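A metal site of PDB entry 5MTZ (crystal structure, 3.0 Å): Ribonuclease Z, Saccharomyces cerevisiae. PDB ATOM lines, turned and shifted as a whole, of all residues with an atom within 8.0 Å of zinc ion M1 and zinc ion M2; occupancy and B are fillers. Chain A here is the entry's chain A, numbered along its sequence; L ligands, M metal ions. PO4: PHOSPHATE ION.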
ATOM      1  N   GLY A 510     -17.866  12.798   1.177  1.00  0.00           N
ATOM      2  CA  GLY A 510     -16.731  13.558   1.695  1.00  0.00           C
ATOM      3  C   GLY A 510     -16.685  13.809   3.193  1.00  0.00           C
ATOM      4  O   GLY A 510     -17.692  13.704   3.896  1.00  0.00           O
ATOM      5  N   SER A 511     -15.501  14.172   3.650  1.00  0.00           N
ATOM      6  CA  SER A 511     -15.237  14.403   5.073  1.00  0.00           C
ATOM      7  C   SER A 511     -15.310  15.879   5.428  1.00  0.00           C
ATOM      8  O   SER A 511     -14.753  16.705   4.726  1.00  0.00           O
ATOM      9  CB  SER A 511     -13.848  13.863   5.451  1.00  0.00           C
ATOM     10  OG  SER A 511     -13.561  14.116   6.826  1.00  0.00           O
ATOM     11  N   ALA A 512     -15.990  16.184   6.529  1.00  0.00           N
ATOM     12  CA  ALA A 512     -15.885  17.488   7.204  1.00  0.00           C
ATOM     13  C   ALA A 512     -16.272  18.712   6.356  1.00  0.00           C
ATOM     14  O   ALA A 512     -17.370  19.245   6.504  1.00  0.00           O
ATOM     15  CB  ALA A 512     -14.483  17.652   7.785  1.00  0.00           C
ATOM     16  N   LEU A 513     -15.362  19.142   5.490  1.00  0.00           N
ATOM     17  CA  LEU A 513     -15.531  20.343   4.644  1.00  0.00           C
ATOM     18  C   LEU A 513     -16.147  19.905   3.329  1.00  0.00           C
ATOM     19  O   LEU A 513     -15.728  18.883   2.787  1.00  0.00           O
ATOM     20  CB  LEU A 513     -14.155  21.025   4.428  1.00  0.00           C
ATOM     21  CG  LEU A 513     -13.820  21.853   3.157  1.00  0.00           C
ATOM     22  CD1 LEU A 513     -12.938  23.052   3.504  1.00  0.00           C
ATOM     23  CD2 LEU A 513     -13.174  21.035   2.023  1.00  0.00           C
ATOM     24  N   VAL A 520     -20.241  17.083   1.379  1.00  0.00           N
ATOM     25  CA  VAL A 520     -20.530  16.358   2.610  1.00  0.00           C
ATOM     26  C   VAL A 520     -21.549  15.199   2.483  1.00  0.00           C
ATOM     27  O   VAL A 520     -22.484  15.232   1.653  1.00  0.00           O
ATOM     28  CB  VAL A 520     -20.968  17.296   3.758  1.00  0.00           C
ATOM     29  CG1 VAL A 520     -19.827  18.206   4.167  1.00  0.00           C
ATOM     30  CG2 VAL A 520     -22.218  18.092   3.390  1.00  0.00           C
ATOM     31  N   VAL A 521     -21.385  14.235   3.382  1.00  0.00           N
ATOM     32  CA  VAL A 521     -21.978  12.885   3.282  1.00  0.00           C
ATOM     33  C   VAL A 521     -23.494  12.870   3.169  1.00  0.00           C
ATOM     34  O   VAL A 521     -24.193  13.642   3.829  1.00  0.00           O
ATOM     35  CB  VAL A 521     -21.718  11.959   4.497  1.00  0.00           C
ATOM     36  CG1 VAL A 521     -21.583  10.503   4.055  1.00  0.00           C
ATOM     37  CG2 VAL A 521     -20.494  12.362   5.317  1.00  0.00           C
ATOM     38  N   ASP A 544     -27.664   9.796   7.166  1.00  0.00           N
ATOM     39  CA  ASP A 544     -27.068  11.137   7.193  1.00  0.00           C
ATOM     40  C   ASP A 544     -27.473  11.978   5.963  1.00  0.00           C
ATOM     41  O   ASP A 544     -28.020  11.463   4.968  1.00  0.00           O
ATOM     42  CB  ASP A 544     -25.534  11.107   7.374  1.00  0.00           C
ATOM     43  CG  ASP A 544     -25.105  10.270   8.584  1.00  0.00           C
ATOM     44  OD1 ASP A 544     -26.007   9.766   9.283  1.00  0.00           O
ATOM     45  OD2 ASP A 544     -23.884  10.104   8.836  1.00  0.00           O
ATOM     46  N   SER A 575     -26.025   9.376  12.302  1.00  0.00           N
ATOM     47  CA  SER A 575     -25.004   8.637  13.037  1.00  0.00           C
ATOM     48  C   SER A 575     -24.543   9.407  14.285  1.00  0.00           C
ATOM     49  O   SER A 575     -24.499   8.831  15.362  1.00  0.00           O
ATOM     50  CB  SER A 575     -23.820   8.332  12.136  1.00  0.00           C
ATOM     51  OG  SER A 575     -23.037   9.492  11.870  1.00  0.00           O
ATOM     52  N   HIS A 576     -24.191  10.671  14.135  1.00  0.00           N
ATOM     53  CA  HIS A 576     -23.736  11.489  15.266  1.00  0.00           C
ATOM     54  C   HIS A 576     -23.896  12.987  15.014  1.00  0.00           C
ATOM     55  O   HIS A 576     -24.353  13.402  13.950  1.00  0.00           O
ATOM     56  CB  HIS A 576     -22.295  11.140  15.623  1.00  0.00           C
ATOM     57  CG  HIS A 576     -21.302  11.456  14.556  1.00  0.00           C
ATOM     58  ND1 HIS A 576     -21.411  10.940  13.286  1.00  0.00           N
ATOM     59  CD2 HIS A 576     -20.178  12.207  14.572  1.00  0.00           C
ATOM     60  CE1 HIS A 576     -20.390  11.368  12.556  1.00  0.00           C
ATOM     61  NE2 HIS A 576     -19.624  12.135  13.310  1.00  0.00           N
ATOM     62  N   LEU A 577     -23.521  13.795  16.003  1.00  0.00           N
ATOM     63  CA  LEU A 577     -23.823  15.224  15.981  1.00  0.00           C
ATOM     64  C   LEU A 577     -22.855  16.126  15.203  1.00  0.00           C
ATOM     65  O   LEU A 577     -23.008  17.350  15.215  1.00  0.00           O
ATOM     66  CB  LEU A 577     -23.971  15.747  17.417  1.00  0.00           C
ATOM     67  CG  LEU A 577     -25.067  15.010  18.182  1.00  0.00           C
ATOM     68  CD1 LEU A 577     -24.837  15.179  19.677  1.00  0.00           C
ATOM     69  CD2 LEU A 577     -26.459  15.477  17.768  1.00  0.00           C
ATOM     70  N   HIS A 578     -21.876  15.559  14.499  1.00  0.00           N
ATOM     71  CA  HIS A 578     -20.998  16.390  13.710  1.00  0.00           C
ATOM     72  C   HIS A 578     -21.778  16.994  12.552  1.00  0.00           C
ATOM     73  O   HIS A 578     -22.598  16.324  11.912  1.00  0.00           O
ATOM     74  CB  HIS A 578     -19.775  15.624  13.221  1.00  0.00           C
ATOM     75  CG  HIS A 578     -18.733  15.415  14.274  1.00  0.00           C
ATOM     76  ND1 HIS A 578     -17.732  14.472  14.156  1.00  0.00           N
ATOM     77  CD2 HIS A 578     -18.548  16.009  15.472  1.00  0.00           C
ATOM     78  CE1 HIS A 578     -16.967  14.516  15.234  1.00  0.00           C
ATOM     79  NE2 HIS A 578     -17.453  15.436  16.053  1.00  0.00           N
ATOM     80  N   ALA A 579     -21.523  18.282  12.325  1.00  0.00           N
ATOM     81  CA  ALA A 579     -22.288  19.092  11.349  1.00  0.00           C
ATOM     82  C   ALA A 579     -22.196  18.585   9.884  1.00  0.00           C
ATOM     83  O   ALA A 579     -23.144  18.801   9.113  1.00  0.00           O
ATOM     84  CB  ALA A 579     -21.857  20.561  11.456  1.00  0.00           C
ATOM     85  N   ASP A 580     -21.099  17.882   9.538  1.00  0.00           N
ATOM     86  CA  ASP A 580     -20.965  17.290   8.196  1.00  0.00           C
ATOM     87  C   ASP A 580     -21.946  16.161   7.927  1.00  0.00           C
ATOM     88  O   ASP A 580     -22.071  15.745   6.780  1.00  0.00           O
ATOM     89  CB  ASP A 580     -19.519  16.826   7.847  1.00  0.00           C
ATOM     90  CG  ASP A 580     -18.980  15.780   8.811  1.00  0.00           C
ATOM     91  OD1 ASP A 580     -19.098  16.045  10.017  1.00  0.00           O
ATOM     92  OD2 ASP A 580     -18.421  14.713   8.400  1.00  0.00           O
ATOM     93  N   HIS A 581     -22.658  15.690   8.958  1.00  0.00           N
ATOM     94  CA  HIS A 581     -23.642  14.614   8.789  1.00  0.00           C
ATOM     95  C   HIS A 581     -25.111  14.997   8.868  1.00  0.00           C
ATOM     96  O   HIS A 581     -25.944  14.240   8.373  1.00  0.00           O
ATOM     97  CB  HIS A 581     -23.364  13.462   9.744  1.00  0.00           C
ATOM     98  CG  HIS A 581     -22.020  12.850   9.533  1.00  0.00           C
ATOM     99  ND1 HIS A 581     -21.824  11.678   8.837  1.00  0.00           N
ATOM    100  CD2 HIS A 581     -20.786  13.304   9.854  1.00  0.00           C
ATOM    101  CE1 HIS A 581     -20.536  11.415   8.774  1.00  0.00           C
ATOM    102  NE2 HIS A 581     -19.879  12.399   9.378  1.00  0.00           N
ATOM    103  N   HIS A 706     -15.609   7.404  18.325  1.00  0.00           N
ATOM    104  CA  HIS A 706     -15.440   8.661  17.621  1.00  0.00           C
ATOM    105  C   HIS A 706     -15.757   9.806  18.575  1.00  0.00           C
ATOM    106  O   HIS A 706     -14.863  10.330  19.257  1.00  0.00           O
ATOM    107  CB  HIS A 706     -16.316   8.658  16.353  1.00  0.00           C
ATOM    108  CG  HIS A 706     -16.234   9.892  15.517  1.00  0.00           C
ATOM    109  ND1 HIS A 706     -15.047  10.379  15.013  1.00  0.00           N
ATOM    110  CD2 HIS A 706     -17.204  10.735  15.072  1.00  0.00           C
ATOM    111  CE1 HIS A 706     -15.278  11.470  14.302  1.00  0.00           C
ATOM    112  NE2 HIS A 706     -16.580  11.702  14.302  1.00  0.00           N
ATOM    113  N   CYS A 707     -17.036  10.124  18.665  1.00  0.00           N
ATOM    114  CA  CYS A 707     -17.539  11.253  19.429  1.00  0.00           C
ATOM    115  C   CYS A 707     -18.260  10.588  20.611  1.00  0.00           C
ATOM    116  O   CYS A 707     -18.508   9.385  20.568  1.00  0.00           O
ATOM    117  CB  CYS A 707     -18.497  12.055  18.507  1.00  0.00           C
ATOM    118  SG  CYS A 707     -19.246  13.576  19.115  1.00  0.00           S
ATOM    119  N   ALA A 710     -21.936   8.959  19.486  1.00  0.00           N
ATOM    120  CA  ALA A 710     -21.831   8.518  18.107  1.00  0.00           C
ATOM    121  C   ALA A 710     -22.370   7.103  18.030  1.00  0.00           C
ATOM    122  O   ALA A 710     -22.555   6.447  19.071  1.00  0.00           O
ATOM    123  CB  ALA A 710     -20.405   8.580  17.635  1.00  0.00           C
ATOM    124  N   TYR A 732     -24.147   0.507   8.619  1.00  0.00           N
ATOM    125  CA  TYR A 732     -23.527   1.806   8.334  1.00  0.00           C
ATOM    126  C   TYR A 732     -22.778   2.288   9.530  1.00  0.00           C
ATOM    127  O   TYR A 732     -23.354   2.560  10.566  1.00  0.00           O
ATOM    128  CB  TYR A 732     -24.585   2.859   7.922  1.00  0.00           C
ATOM    129  CG  TYR A 732     -24.066   4.291   7.716  1.00  0.00           C
ATOM    130  CD1 TYR A 732     -22.904   4.551   7.004  1.00  0.00           C
ATOM    131  CD2 TYR A 732     -24.775   5.380   8.210  1.00  0.00           C
ATOM    132  CE1 TYR A 732     -22.438   5.846   6.817  1.00  0.00           C
ATOM    133  CE2 TYR A 732     -24.309   6.685   8.026  1.00  0.00           C
ATOM    134  CZ  TYR A 732     -23.143   6.910   7.323  1.00  0.00           C
ATOM    135  OH  TYR A 732     -22.670   8.186   7.126  1.00  0.00           O
ATOM    136  N   GLY A 734     -20.667   5.055  11.650  1.00  0.00           N
ATOM    137  CA  GLY A 734     -20.687   6.499  11.788  1.00  0.00           C
ATOM    138  C   GLY A 734     -19.437   7.073  11.152  1.00  0.00           C
ATOM    139  O   GLY A 734     -19.190   6.909   9.951  1.00  0.00           O
ATOM    140  N   ASP A 735     -18.669   7.773  11.984  1.00  0.00           N
ATOM    141  CA  ASP A 735     -17.319   8.164  11.663  1.00  0.00           C
ATOM    142  C   ASP A 735     -16.453   7.319  12.618  1.00  0.00           C
ATOM    143  O   ASP A 735     -15.530   7.837  13.240  1.00  0.00           O
ATOM    144  CB  ASP A 735     -17.121   9.675  11.917  1.00  0.00           C
ATOM    145  CG  ASP A 735     -17.611  10.593  10.773  1.00  0.00           C
ATOM    146  OD1 ASP A 735     -17.965  10.045   9.719  1.00  0.00           O
ATOM    147  OD2 ASP A 735     -17.628  11.863  10.962  1.00  0.00           O
ATOM    148  N   THR A 736     -16.734   6.028  12.729  1.00  0.00           N
ATOM    149  CA  THR A 736     -16.085   5.213  13.764  1.00  0.00           C
ATOM    150  C   THR A 736     -14.615   4.951  13.432  1.00  0.00           C
ATOM    151  O   THR A 736     -14.192   4.923  12.274  1.00  0.00           O
ATOM    152  CB  THR A 736     -16.850   3.882  14.063  1.00  0.00           C
ATOM    153  OG1 THR A 736     -16.471   3.372  15.354  1.00  0.00           O
ATOM    154  CG2 THR A 736     -16.625   2.812  12.968  1.00  0.00           C
ATOM    155  N   GLU A 757     -17.179   4.006   6.515  1.00  0.00           N
ATOM    156  CA  GLU A 757     -16.374   5.210   6.439  1.00  0.00           C
ATOM    157  C   GLU A 757     -14.952   4.872   6.065  1.00  0.00           C
ATOM    158  O   GLU A 757     -14.342   4.001   6.685  1.00  0.00           O
ATOM    159  CB  GLU A 757     -16.433   5.880   7.811  1.00  0.00           C
ATOM    160  CG  GLU A 757     -15.577   7.124   7.992  1.00  0.00           C
ATOM    161  CD  GLU A 757     -14.372   6.868   8.834  1.00  0.00           C
ATOM    162  OE1 GLU A 757     -13.392   6.345   8.294  1.00  0.00           O
ATOM    163  OE2 GLU A 757     -14.404   7.208  10.043  1.00  0.00           O
ATOM    164  N   THR A 759     -12.296   7.515   5.549  1.00  0.00           N
ATOM    165  CA  THR A 759     -11.797   8.892   5.527  1.00  0.00           C
ATOM    166  C   THR A 759     -10.404   8.969   4.949  1.00  0.00           C
ATOM    167  O   THR A 759     -10.204   9.556   3.888  1.00  0.00           O
ATOM    168  CB  THR A 759     -11.825   9.543   6.948  1.00  0.00           C
ATOM    169  OG1 THR A 759     -13.126   9.380   7.536  1.00  0.00           O
ATOM    170  CG2 THR A 759     -11.540  11.030   6.883  1.00  0.00           C
ATOM    171  N   LYS A 771      -7.686  11.632  14.793  1.00  0.00           N
ATOM    172  CA  LYS A 771      -8.970  12.146  14.327  1.00  0.00           C
ATOM    173  C   LYS A 771     -10.140  11.143  14.422  1.00  0.00           C
ATOM    174  O   LYS A 771     -11.280  11.523  14.167  1.00  0.00           O
ATOM    175  CB  LYS A 771      -8.837  12.648  12.887  1.00  0.00           C
ATOM    176  CG  LYS A 771      -8.029  13.940  12.796  1.00  0.00           C
ATOM    177  CD  LYS A 771      -7.897  14.392  11.350  1.00  0.00           C
ATOM    178  CE  LYS A 771      -7.386  15.814  11.281  1.00  0.00           C
ATOM    179  NZ  LYS A 771      -7.402  16.291   9.872  1.00  0.00           N
ATOM    180  N   LYS A 772      -9.837   9.895  14.772  1.00  0.00           N
ATOM    181  CA  LYS A 772     -10.822   8.825  15.051  1.00  0.00           C
ATOM    182  C   LYS A 772     -11.667   8.433  13.837  1.00  0.00           C
ATOM    183  O   LYS A 772     -12.885   8.325  13.919  1.00  0.00           O
ATOM    184  CB  LYS A 772     -11.663   9.138  16.315  1.00  0.00           C
ATOM    185  CG  LYS A 772     -10.959   8.695  17.585  1.00  0.00           C
ATOM    186  CD  LYS A 772     -11.729   8.997  18.861  1.00  0.00           C
ATOM    187  CE  LYS A 772     -11.429  10.391  19.384  1.00  0.00           C
ATOM    188  NZ  LYS A 772     -12.315  10.761  20.515  1.00  0.00           N
ATOM    189  N   HIS A 773     -10.990   8.201  12.706  1.00  0.00           N
ATOM    190  CA  HIS A 773     -11.580   7.612  11.496  1.00  0.00           C
ATOM    191  C   HIS A 773     -10.776   6.398  11.067  1.00  0.00           C
ATOM    192  O   HIS A 773      -9.595   6.310  11.386  1.00  0.00           O
ATOM    193  CB  HIS A 773     -11.564   8.600  10.326  1.00  0.00           C
ATOM    194  CG  HIS A 773     -12.369   9.841  10.571  1.00  0.00           C
ATOM    195  ND1 HIS A 773     -13.711   9.916  10.280  1.00  0.00           N
ATOM    196  CD2 HIS A 773     -12.014  11.043  11.082  1.00  0.00           C
ATOM    197  CE1 HIS A 773     -14.159  11.116  10.601  1.00  0.00           C
ATOM    198  NE2 HIS A 773     -13.152  11.814  11.093  1.00  0.00           N
ATOM    199  N   HIS A 795     -17.398   8.841   2.644  1.00  0.00           N
ATOM    200  CA  HIS A 795     -16.836   9.742   3.646  1.00  0.00           C
ATOM    201  C   HIS A 795     -15.321   9.806   3.469  1.00  0.00           C
ATOM    202  O   HIS A 795     -14.563   9.547   4.407  1.00  0.00           O
ATOM    203  CB  HIS A 795     -17.208   9.304   5.060  1.00  0.00           C
ATOM    204  CG  HIS A 795     -16.960  10.343   6.095  1.00  0.00           C
ATOM    205  ND1 HIS A 795     -15.696  10.785   6.409  1.00  0.00           N
ATOM    206  CD2 HIS A 795     -17.811  11.038   6.882  1.00  0.00           C
ATOM    207  CE1 HIS A 795     -15.786  11.710   7.350  1.00  0.00           C
ATOM    208  NE2 HIS A 795     -17.062  11.887   7.650  1.00  0.00           N
HETATM  209  P   PO4 L   1     -15.546  14.495  10.841  1.00  0.00           P
HETATM  210  O1  PO4 L   1     -15.874  13.721  12.105  1.00  0.00           O
HETATM  211  O2  PO4 L   1     -15.902  13.727   9.584  1.00  0.00           O
HETATM  212  O3  PO4 L   1     -14.083  14.876  10.846  1.00  0.00           O
HETATM  213  O4  PO4 L   1     -16.357  15.753  10.832  1.00  0.00           O
HETATM  214 ZN    ZN M   1     -17.716  12.976   9.229  1.00  0.00          ZN
HETATM  215 ZN    ZN M   2     -17.642  12.990  12.708  1.00  0.00          ZN
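The nearest printed residue that does not touch zinc ion M2 is His 581 (4.1 Å).
Four residues have an atom within 4 Å of zinc ion M1: Asp 580, His 581, Asp 735 and His 795.
ND1 of His 576 is in hydrogen-bond range of OG of Ser 575 (2.6 Å).
N of Ala 512 lies close to OD2 of Asp 580, 3.4 Å away.
A ring nitrogen (ND1) of His 581 is in hydrogen-bond range of the side-chain carboxylate (OD2) of Asp 544 (2.6 Å).
The side-chain hydroxyl (OG1) of Thr 759 sits at hydrogen-bond distance from a ring nitrogen (ND1) of His 795 (3.1 Å).
The side-chain amino group (NZ) of Lys 772 sits at hydrogen-bond distance from the backbone carbonyl oxygen (O) of His 706 (2.9 Å).
Zinc ion M2 is bound by an oxygen (O1) of the ligand, a ring nitrogen (ND1) of His 578, the side-chain carboxylate (OD2) of Asp 735, a ring nitrogen (NE2) of His 576 and a ring nitrogen (NE2) of His 706.
O2 of the ligand binds zinc ion M1.
NE2 of His 795 binds zinc ion M1 (2.0 Å).
OD2 of Asp 580 binds zinc ion M1 (2.0 Å).
OD2 of Asp 735 binds zinc ion M1, 2.1 Å away.
A ring nitrogen (NE2) of His 581 binds zinc ion M1 (2.2 Å).
Zinc ion M1 has five donor atoms within binding distance.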
